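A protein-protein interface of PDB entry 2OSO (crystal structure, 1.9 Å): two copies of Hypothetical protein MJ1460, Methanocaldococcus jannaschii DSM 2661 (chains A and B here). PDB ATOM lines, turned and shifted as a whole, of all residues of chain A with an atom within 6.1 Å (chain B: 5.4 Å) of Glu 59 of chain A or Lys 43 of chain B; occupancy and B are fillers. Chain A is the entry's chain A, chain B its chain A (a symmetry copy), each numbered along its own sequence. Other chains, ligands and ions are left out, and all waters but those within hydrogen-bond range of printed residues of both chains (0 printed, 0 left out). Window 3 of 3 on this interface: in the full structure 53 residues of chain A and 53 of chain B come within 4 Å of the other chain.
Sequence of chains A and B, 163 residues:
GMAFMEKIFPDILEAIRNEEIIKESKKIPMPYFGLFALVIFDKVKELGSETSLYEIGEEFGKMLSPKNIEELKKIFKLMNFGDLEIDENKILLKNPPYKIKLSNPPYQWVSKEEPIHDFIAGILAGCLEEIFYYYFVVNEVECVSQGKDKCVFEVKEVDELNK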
ATOM      1  N   SER A  49     -37.973  22.356  21.890  1.00  0.00           N
ATOM      2  CA  SER A  49     -36.917  22.227  20.865  1.00  0.00           C
ATOM      3  C   SER A  49     -35.945  21.051  21.144  1.00  0.00           C
ATOM      4  O   SER A  49     -36.317  20.107  21.859  1.00  0.00           O
ATOM      5  CB  SER A  49     -36.176  23.557  20.692  1.00  0.00           C
ATOM      6  N   THR A  51     -31.379  19.749  20.764  1.00  0.00           N
ATOM      7  CA  THR A  51     -29.935  19.974  20.405  1.00  0.00           C
ATOM      8  C   THR A  51     -29.070  18.771  20.862  1.00  0.00           C
ATOM      9  O   THR A  51     -29.611  17.704  21.159  1.00  0.00           O
ATOM     10  CB  THR A  51     -29.411  21.390  20.917  1.00  0.00           C
ATOM     11  OG1 THR A  51     -28.093  21.666  20.394  1.00  0.00           O
ATOM     12  CG2 THR A  51     -29.438  21.481  22.430  1.00  0.00           C
ATOM     13  N   TYR A  54     -22.672  17.590  21.820  1.00  0.00           N
ATOM     14  CA  TYR A  54     -21.670  17.921  20.805  1.00  0.00           C
ATOM     15  C   TYR A  54     -21.904  19.313  20.233  1.00  0.00           C
ATOM     16  O   TYR A  54     -20.994  20.136  20.170  1.00  0.00           O
ATOM     17  CB  TYR A  54     -21.725  16.901  19.695  1.00  0.00           C
ATOM     18  CG  TYR A  54     -20.677  17.112  18.622  1.00  0.00           C
ATOM     19  CD1 TYR A  54     -19.405  16.642  18.791  1.00  0.00           C
ATOM     20  CD2 TYR A  54     -20.982  17.759  17.443  1.00  0.00           C
ATOM     21  CE1 TYR A  54     -18.417  16.839  17.827  1.00  0.00           C
ATOM     22  CE2 TYR A  54     -19.989  17.963  16.451  1.00  0.00           C
ATOM     23  CZ  TYR A  54     -18.712  17.475  16.652  1.00  0.00           C
ATOM     24  OH  TYR A  54     -17.691  17.668  15.707  1.00  0.00           O
ATOM     25  N   GLU A  55     -23.110  19.602  19.819  1.00  0.00           N
ATOM     26  CA  GLU A  55     -23.368  20.917  19.243  1.00  0.00           C
ATOM     27  C   GLU A  55     -23.198  22.067  20.236  1.00  0.00           C
ATOM     28  O   GLU A  55     -22.622  23.101  19.910  1.00  0.00           O
ATOM     29  CB  GLU A  55     -24.743  20.932  18.600  1.00  0.00           C
ATOM     30  CG  GLU A  55     -24.811  20.031  17.391  1.00  0.00           C
ATOM     31  CD  GLU A  55     -26.223  19.873  16.893  1.00  0.00           C
ATOM     32  OE1 GLU A  55     -26.931  20.922  16.801  1.00  0.00           O
ATOM     33  OE2 GLU A  55     -26.594  18.706  16.597  1.00  0.00           O
ATOM     34  N   ILE A  56     -23.631  21.874  21.479  1.00  0.00           N
ATOM     35  CA  ILE A  56     -23.325  22.824  22.534  1.00  0.00           C
ATOM     36  C   ILE A  56     -21.817  23.010  22.804  1.00  0.00           C
ATOM     37  O   ILE A  56     -21.348  24.123  23.031  1.00  0.00           O
ATOM     38  CB  ILE A  56     -24.099  22.471  23.869  1.00  0.00           C
ATOM     39  CG1 ILE A  56     -25.612  22.379  23.641  1.00  0.00           C
ATOM     40  CG2 ILE A  56     -23.790  23.510  24.962  1.00  0.00           C
ATOM     41  CD1 ILE A  56     -26.249  23.779  23.341  1.00  0.00           C
ATOM     42  N   GLY A  57     -21.049  21.930  22.844  1.00  0.00           N
ATOM     43  CA  GLY A  57     -19.590  21.996  22.906  1.00  0.00           C
ATOM     44  C   GLY A  57     -18.984  22.786  21.760  1.00  0.00           C
ATOM     45  O   GLY A  57     -18.128  23.653  21.991  1.00  0.00           O
ATOM     46  N   GLU A  58     -19.473  22.571  20.541  1.00  0.00           N
ATOM     47  CA  GLU A  58     -19.033  23.437  19.406  1.00  0.00           C
ATOM     48  C   GLU A  58     -19.185  24.901  19.714  1.00  0.00           C
ATOM     49  O   GLU A  58     -18.254  25.682  19.545  1.00  0.00           O
ATOM     50  CB  GLU A  58     -19.755  23.127  18.084  1.00  0.00           C
ATOM     51  CG  GLU A  58     -19.508  21.710  17.557  1.00  0.00           C
ATOM     52  CD  GLU A  58     -20.242  21.474  16.267  1.00  0.00           C
ATOM     53  OE1 GLU A  58     -21.443  21.166  16.345  1.00  0.00           O
ATOM     54  OE2 GLU A  58     -19.619  21.607  15.190  1.00  0.00           O
ATOM     55  N   GLU A  59     -20.368  25.291  20.192  1.00  0.00           N
ATOM     56  CA  GLU A  59     -20.630  26.716  20.510  1.00  0.00           C
ATOM     57  C   GLU A  59     -19.793  27.230  21.683  1.00  0.00           C
ATOM     58  O   GLU A  59     -19.359  28.354  21.667  1.00  0.00           O
ATOM     59  CB  GLU A  59     -22.122  26.954  20.820  1.00  0.00           C
ATOM     60  CG  GLU A  59     -23.043  26.684  19.670  1.00  0.00           C
ATOM     61  CD  GLU A  59     -22.911  27.684  18.513  1.00  0.00           C
ATOM     62  OE1 GLU A  59     -22.153  28.693  18.556  1.00  0.00           O
ATOM     63  OE2 GLU A  59     -23.597  27.423  17.519  1.00  0.00           O
ATOM     64  N   PHE A  60     -19.611  26.375  22.685  1.00  0.00           N
ATOM     65  CA  PHE A  60     -18.783  26.616  23.864  1.00  0.00           C
ATOM     66  C   PHE A  60     -17.348  26.908  23.431  1.00  0.00           C
ATOM     67  O   PHE A  60     -16.792  27.948  23.803  1.00  0.00           O
ATOM     68  CB  PHE A  60     -18.881  25.405  24.770  1.00  0.00           C
ATOM     69  CG  PHE A  60     -18.418  25.626  26.173  1.00  0.00           C
ATOM     70  CD1 PHE A  60     -17.096  25.465  26.491  1.00  0.00           C
ATOM     71  CD2 PHE A  60     -19.349  25.903  27.197  1.00  0.00           C
ATOM     72  CE1 PHE A  60     -16.658  25.591  27.810  1.00  0.00           C
ATOM     73  CE2 PHE A  60     -18.950  26.046  28.471  1.00  0.00           C
ATOM     74  CZ  PHE A  60     -17.597  25.897  28.808  1.00  0.00           C
ATOM     75  N   GLY A  61     -16.843  26.063  22.539  1.00  0.00           N
ATOM     76  CA  GLY A  61     -15.513  26.194  21.935  1.00  0.00           C
ATOM     77  C   GLY A  61     -15.308  27.502  21.222  1.00  0.00           C
ATOM     78  O   GLY A  61     -14.297  28.190  21.437  1.00  0.00           O
ATOM     79  N   LYS A  62     -16.300  27.889  20.413  1.00  0.00           N
ATOM     80  CA  LYS A  62     -16.322  29.200  19.752  1.00  0.00           C
ATOM     81  C   LYS A  62     -16.287  30.404  20.707  1.00  0.00           C
ATOM     82  O   LYS A  62     -15.497  31.313  20.500  1.00  0.00           O
ATOM     83  CB  LYS A  62     -17.524  29.318  18.796  1.00  0.00           C
ATOM     84  CG  LYS A  62     -17.558  28.304  17.621  1.00  0.00           C
ATOM     85  CD  LYS A  62     -16.210  28.166  16.985  1.00  0.00           C
ATOM     86  CE  LYS A  62     -16.226  27.573  15.622  1.00  0.00           C
ATOM     87  N   MET A  63     -17.135  30.415  21.738  1.00  0.00           N
ATOM     88  CA  MET A  63     -17.032  31.412  22.798  1.00  0.00           C
ATOM     89  C   MET A  63     -15.617  31.495  23.410  1.00  0.00           C
ATOM     90  O   MET A  63     -15.119  32.601  23.656  1.00  0.00           O
ATOM     91  CB  MET A  63     -18.056  31.151  23.930  1.00  0.00           C
ATOM     92  CG  MET A  63     -19.394  31.926  23.861  1.00  0.00           C
ATOM     93  SD  MET A  63     -19.304  33.862  23.598  1.00  0.00           S
ATOM     94  CE  MET A  63     -17.560  34.268  24.380  1.00  0.00           C
ATOM     95  N   LEU A  64     -14.987  30.352  23.675  1.00  0.00           N
ATOM     96  CA  LEU A  64     -13.686  30.320  24.336  1.00  0.00           C
ATOM     97  C   LEU A  64     -12.634  30.929  23.411  1.00  0.00           C
ATOM     98  O   LEU A  64     -11.757  31.686  23.838  1.00  0.00           O
ATOM     99  CB  LEU A  64     -13.277  28.881  24.704  1.00  0.00           C
ATOM    100  CG  LEU A  64     -14.026  28.114  25.788  1.00  0.00           C
ATOM    101  CD1 LEU A  64     -13.557  26.654  25.758  1.00  0.00           C
ATOM    102  CD2 LEU A  64     -13.847  28.736  27.144  1.00  0.00           C
ATOM    103  N   GLY A 122     -17.093  18.267  20.841  1.00  0.00           N
ATOM    104  CA  GLY A 122     -17.666  19.494  20.287  1.00  0.00           C
ATOM    105  C   GLY A 122     -16.786  20.670  20.579  1.00  0.00           C
ATOM    106  O   GLY A 122     -16.537  21.571  19.702  1.00  0.00           O
ATOM    107  N   GLY A 126     -14.998  23.207  17.821  1.00  0.00           N
ATOM    108  CA  GLY A 126     -15.232  24.623  17.838  1.00  0.00           C
ATOM    109  C   GLY A 126     -13.960  25.418  18.006  1.00  0.00           C
ATOM    110  O   GLY A 126     -13.777  26.459  17.343  1.00  0.00           O
ATOM    111  N   VAL B  39     -24.252  29.567  26.923  1.00  0.00           N
ATOM    112  CA  VAL B  39     -24.233  29.004  25.564  1.00  0.00           C
ATOM    113  C   VAL B  39     -25.555  28.272  25.241  1.00  0.00           C
ATOM    114  O   VAL B  39     -26.099  28.449  24.159  1.00  0.00           O
ATOM    115  CB  VAL B  39     -22.959  28.137  25.293  1.00  0.00           C
ATOM    116  CG1 VAL B  39     -23.103  27.347  23.994  1.00  0.00           C
ATOM    117  CG2 VAL B  39     -21.682  29.026  25.308  1.00  0.00           C
ATOM    118  N   ILE B  40     -26.080  27.494  26.180  1.00  0.00           N
ATOM    119  CA  ILE B  40     -27.319  26.762  25.924  1.00  0.00           C
ATOM    120  C   ILE B  40     -28.603  27.614  25.990  1.00  0.00           C
ATOM    121  O   ILE B  40     -29.636  27.168  25.493  1.00  0.00           O
ATOM    122  CB  ILE B  40     -27.453  25.488  26.791  1.00  0.00           C
ATOM    123  CG1 ILE B  40     -28.467  24.516  26.164  1.00  0.00           C
ATOM    124  CG2 ILE B  40     -27.871  25.795  28.231  1.00  0.00           C
ATOM    125  CD1 ILE B  40     -28.516  23.234  26.882  1.00  0.00           C
ATOM    126  N   PHE B  41     -28.549  28.805  26.600  1.00  0.00           N
ATOM    127  CA  PHE B  41     -29.640  29.759  26.500  1.00  0.00           C
ATOM    128  C   PHE B  41     -29.675  30.437  25.137  1.00  0.00           C
ATOM    129  O   PHE B  41     -30.744  30.711  24.621  1.00  0.00           O
ATOM    130  CB  PHE B  41     -29.575  30.827  27.601  1.00  0.00           C
ATOM    131  CG  PHE B  41     -30.212  30.411  28.903  1.00  0.00           C
ATOM    132  CD1 PHE B  41     -29.895  29.210  29.492  1.00  0.00           C
ATOM    133  CD2 PHE B  41     -31.112  31.250  29.547  1.00  0.00           C
ATOM    134  CE1 PHE B  41     -30.469  28.840  30.691  1.00  0.00           C
ATOM    135  CE2 PHE B  41     -31.682  30.904  30.751  1.00  0.00           C
ATOM    136  CZ  PHE B  41     -31.359  29.694  31.331  1.00  0.00           C
ATOM    137  N   ASP B  42     -28.517  30.746  24.572  1.00  0.00           N
ATOM    138  CA  ASP B  42     -28.449  31.190  23.178  1.00  0.00           C
ATOM    139  C   ASP B  42     -29.090  30.191  22.217  1.00  0.00           C
ATOM    140  O   ASP B  42     -29.702  30.597  21.235  1.00  0.00           O
ATOM    141  CB  ASP B  42     -27.011  31.358  22.750  1.00  0.00           C
ATOM    142  CG  ASP B  42     -26.520  32.728  22.951  1.00  0.00           C
ATOM    143  OD1 ASP B  42     -26.857  33.598  22.122  1.00  0.00           O
ATOM    144  OD2 ASP B  42     -25.772  32.946  23.918  1.00  0.00           O
ATOM    145  N   LYS B  43     -28.908  28.899  22.474  1.00  0.00           N
ATOM    146  CA  LYS B  43     -29.541  27.838  21.678  1.00  0.00           C
ATOM    147  C   LYS B  43     -31.024  27.635  22.020  1.00  0.00           C
ATOM    148  O   LYS B  43     -31.827  27.468  21.117  1.00  0.00           O
ATOM    149  CB  LYS B  43     -28.778  26.503  21.844  1.00  0.00           C
ATOM    150  CG  LYS B  43     -27.323  26.544  21.324  1.00  0.00           C
ATOM    151  CD  LYS B  43     -27.074  25.671  20.078  1.00  0.00           C
ATOM    152  CE  LYS B  43     -26.934  26.480  18.795  1.00  0.00           C
ATOM    153  NZ  LYS B  43     -26.717  25.598  17.584  1.00  0.00           N
ATOM    154  N   VAL B  44     -31.385  27.597  23.310  1.00  0.00           N
ATOM    155  CA  VAL B  44     -32.804  27.651  23.708  1.00  0.00           C
ATOM    156  C   VAL B  44     -33.420  28.794  22.890  1.00  0.00           C
ATOM    157  O   VAL B  44     -34.322  28.575  22.087  1.00  0.00           O
ATOM    158  CB  VAL B  44     -33.040  27.874  25.281  1.00  0.00           C
ATOM    159  CG1 VAL B  44     -34.495  28.277  25.605  1.00  0.00           C
ATOM    160  CG2 VAL B  44     -32.623  26.650  26.114  1.00  0.00           C
ATOM    161  N   LYS B  45     -32.905  30.002  23.059  1.00  0.00           N
ATOM    162  CA  LYS B  45     -33.443  31.152  22.325  1.00  0.00           C
ATOM    163  C   LYS B  45     -33.254  30.942  20.836  1.00  0.00           C
ATOM    164  O   LYS B  45     -34.200  31.114  20.064  1.00  0.00           O
ATOM    165  CB  LYS B  45     -32.784  32.478  22.757  1.00  0.00           C
ATOM    166  N   GLY B  48     -35.414  27.846  19.442  1.00  0.00           N
ATOM    167  CA  GLY B  48     -36.546  28.778  19.355  1.00  0.00           C
ATOM    168  C   GLY B  48     -37.497  28.855  20.554  1.00  0.00           C
ATOM    169  O   GLY B  48     -38.648  29.274  20.385  1.00  0.00           O
ATOM    170  N   SER B  49     -37.030  28.483  21.755  1.00  0.00           N
ATOM    171  CA  SER B  49     -37.836  28.578  22.988  1.00  0.00           C
ATOM    172  C   SER B  49     -37.222  29.539  24.039  1.00  0.00           C
ATOM    173  O   SER B  49     -36.436  30.427  23.669  1.00  0.00           O
ATOM    174  CB  SER B  49     -38.094  27.182  23.567  1.00  0.00           C
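NZ of Lys 43 of chain B lies within salt-bridge range of OE2 of Glu 59 of chain A, 3.6 Å away.
Of the printed residues of chain B, Ile 56 of chain A touches Val 39 (3.8 Å), Ile 40 (3.7 Å) and Lys 43 (3.6 Å).
Printed residues of chain A within 4 Å of Val 39 of chain B: Ile 56, Glu 59, Phe 60 and Met 63.
Printed residues of chain B within 4 Å of Met 63 of chain A: Val 39 (3.97 Å).
Of the printed residues of chain A, Ile 40 of chain B touches Ile 56 (3.7 Å).
Of the printed residues of chain B, Phe 60 of chain A touches Val 39 (3.9 Å).
Phe 41 of chain B touches none of the printed residues of chain A.
Glu 58 of chain A touches none of the printed residues of chain B.
The nearest printed residue of chain B that does not touch Glu 59 of chain A is Ile 40 of chain B (6.7 Å).
Position printed for both chains: 49.
Among the printed residues, pairs that only touch across the chains: Ile 56 of chain A with Val 39 of chain B (3.8 Å), Ile 56 of chain A with Ile 40 of chain B (3.7 Å), Ile 56 of chain A with Lys 43 of chain B (3.6 Å), Glu 59 of chain A with Val 39 of chain B (3.3 Å), Phe 60 of chain A with Val 39 of chain B (3.9 Å) and Met 63 of chain A with Val 39 of chain B (3.97 Å).
Printed residues of chain A that touch a printed residue of chain B: Ile 56, Glu 59, Phe 60 and Met 63.
Along chain A the printed residues that touch a printed residue of chain B span positions 56 to 63.
Among the printed residues, 7 pairs touch across the chains.
Among the printed residues, Asp or Glu carboxylates within 4 Å of a Lys or Arg side-chain nitrogen of the other chain: Glu 59 of chain A with Lys 43 of chain B (3.6 Å).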
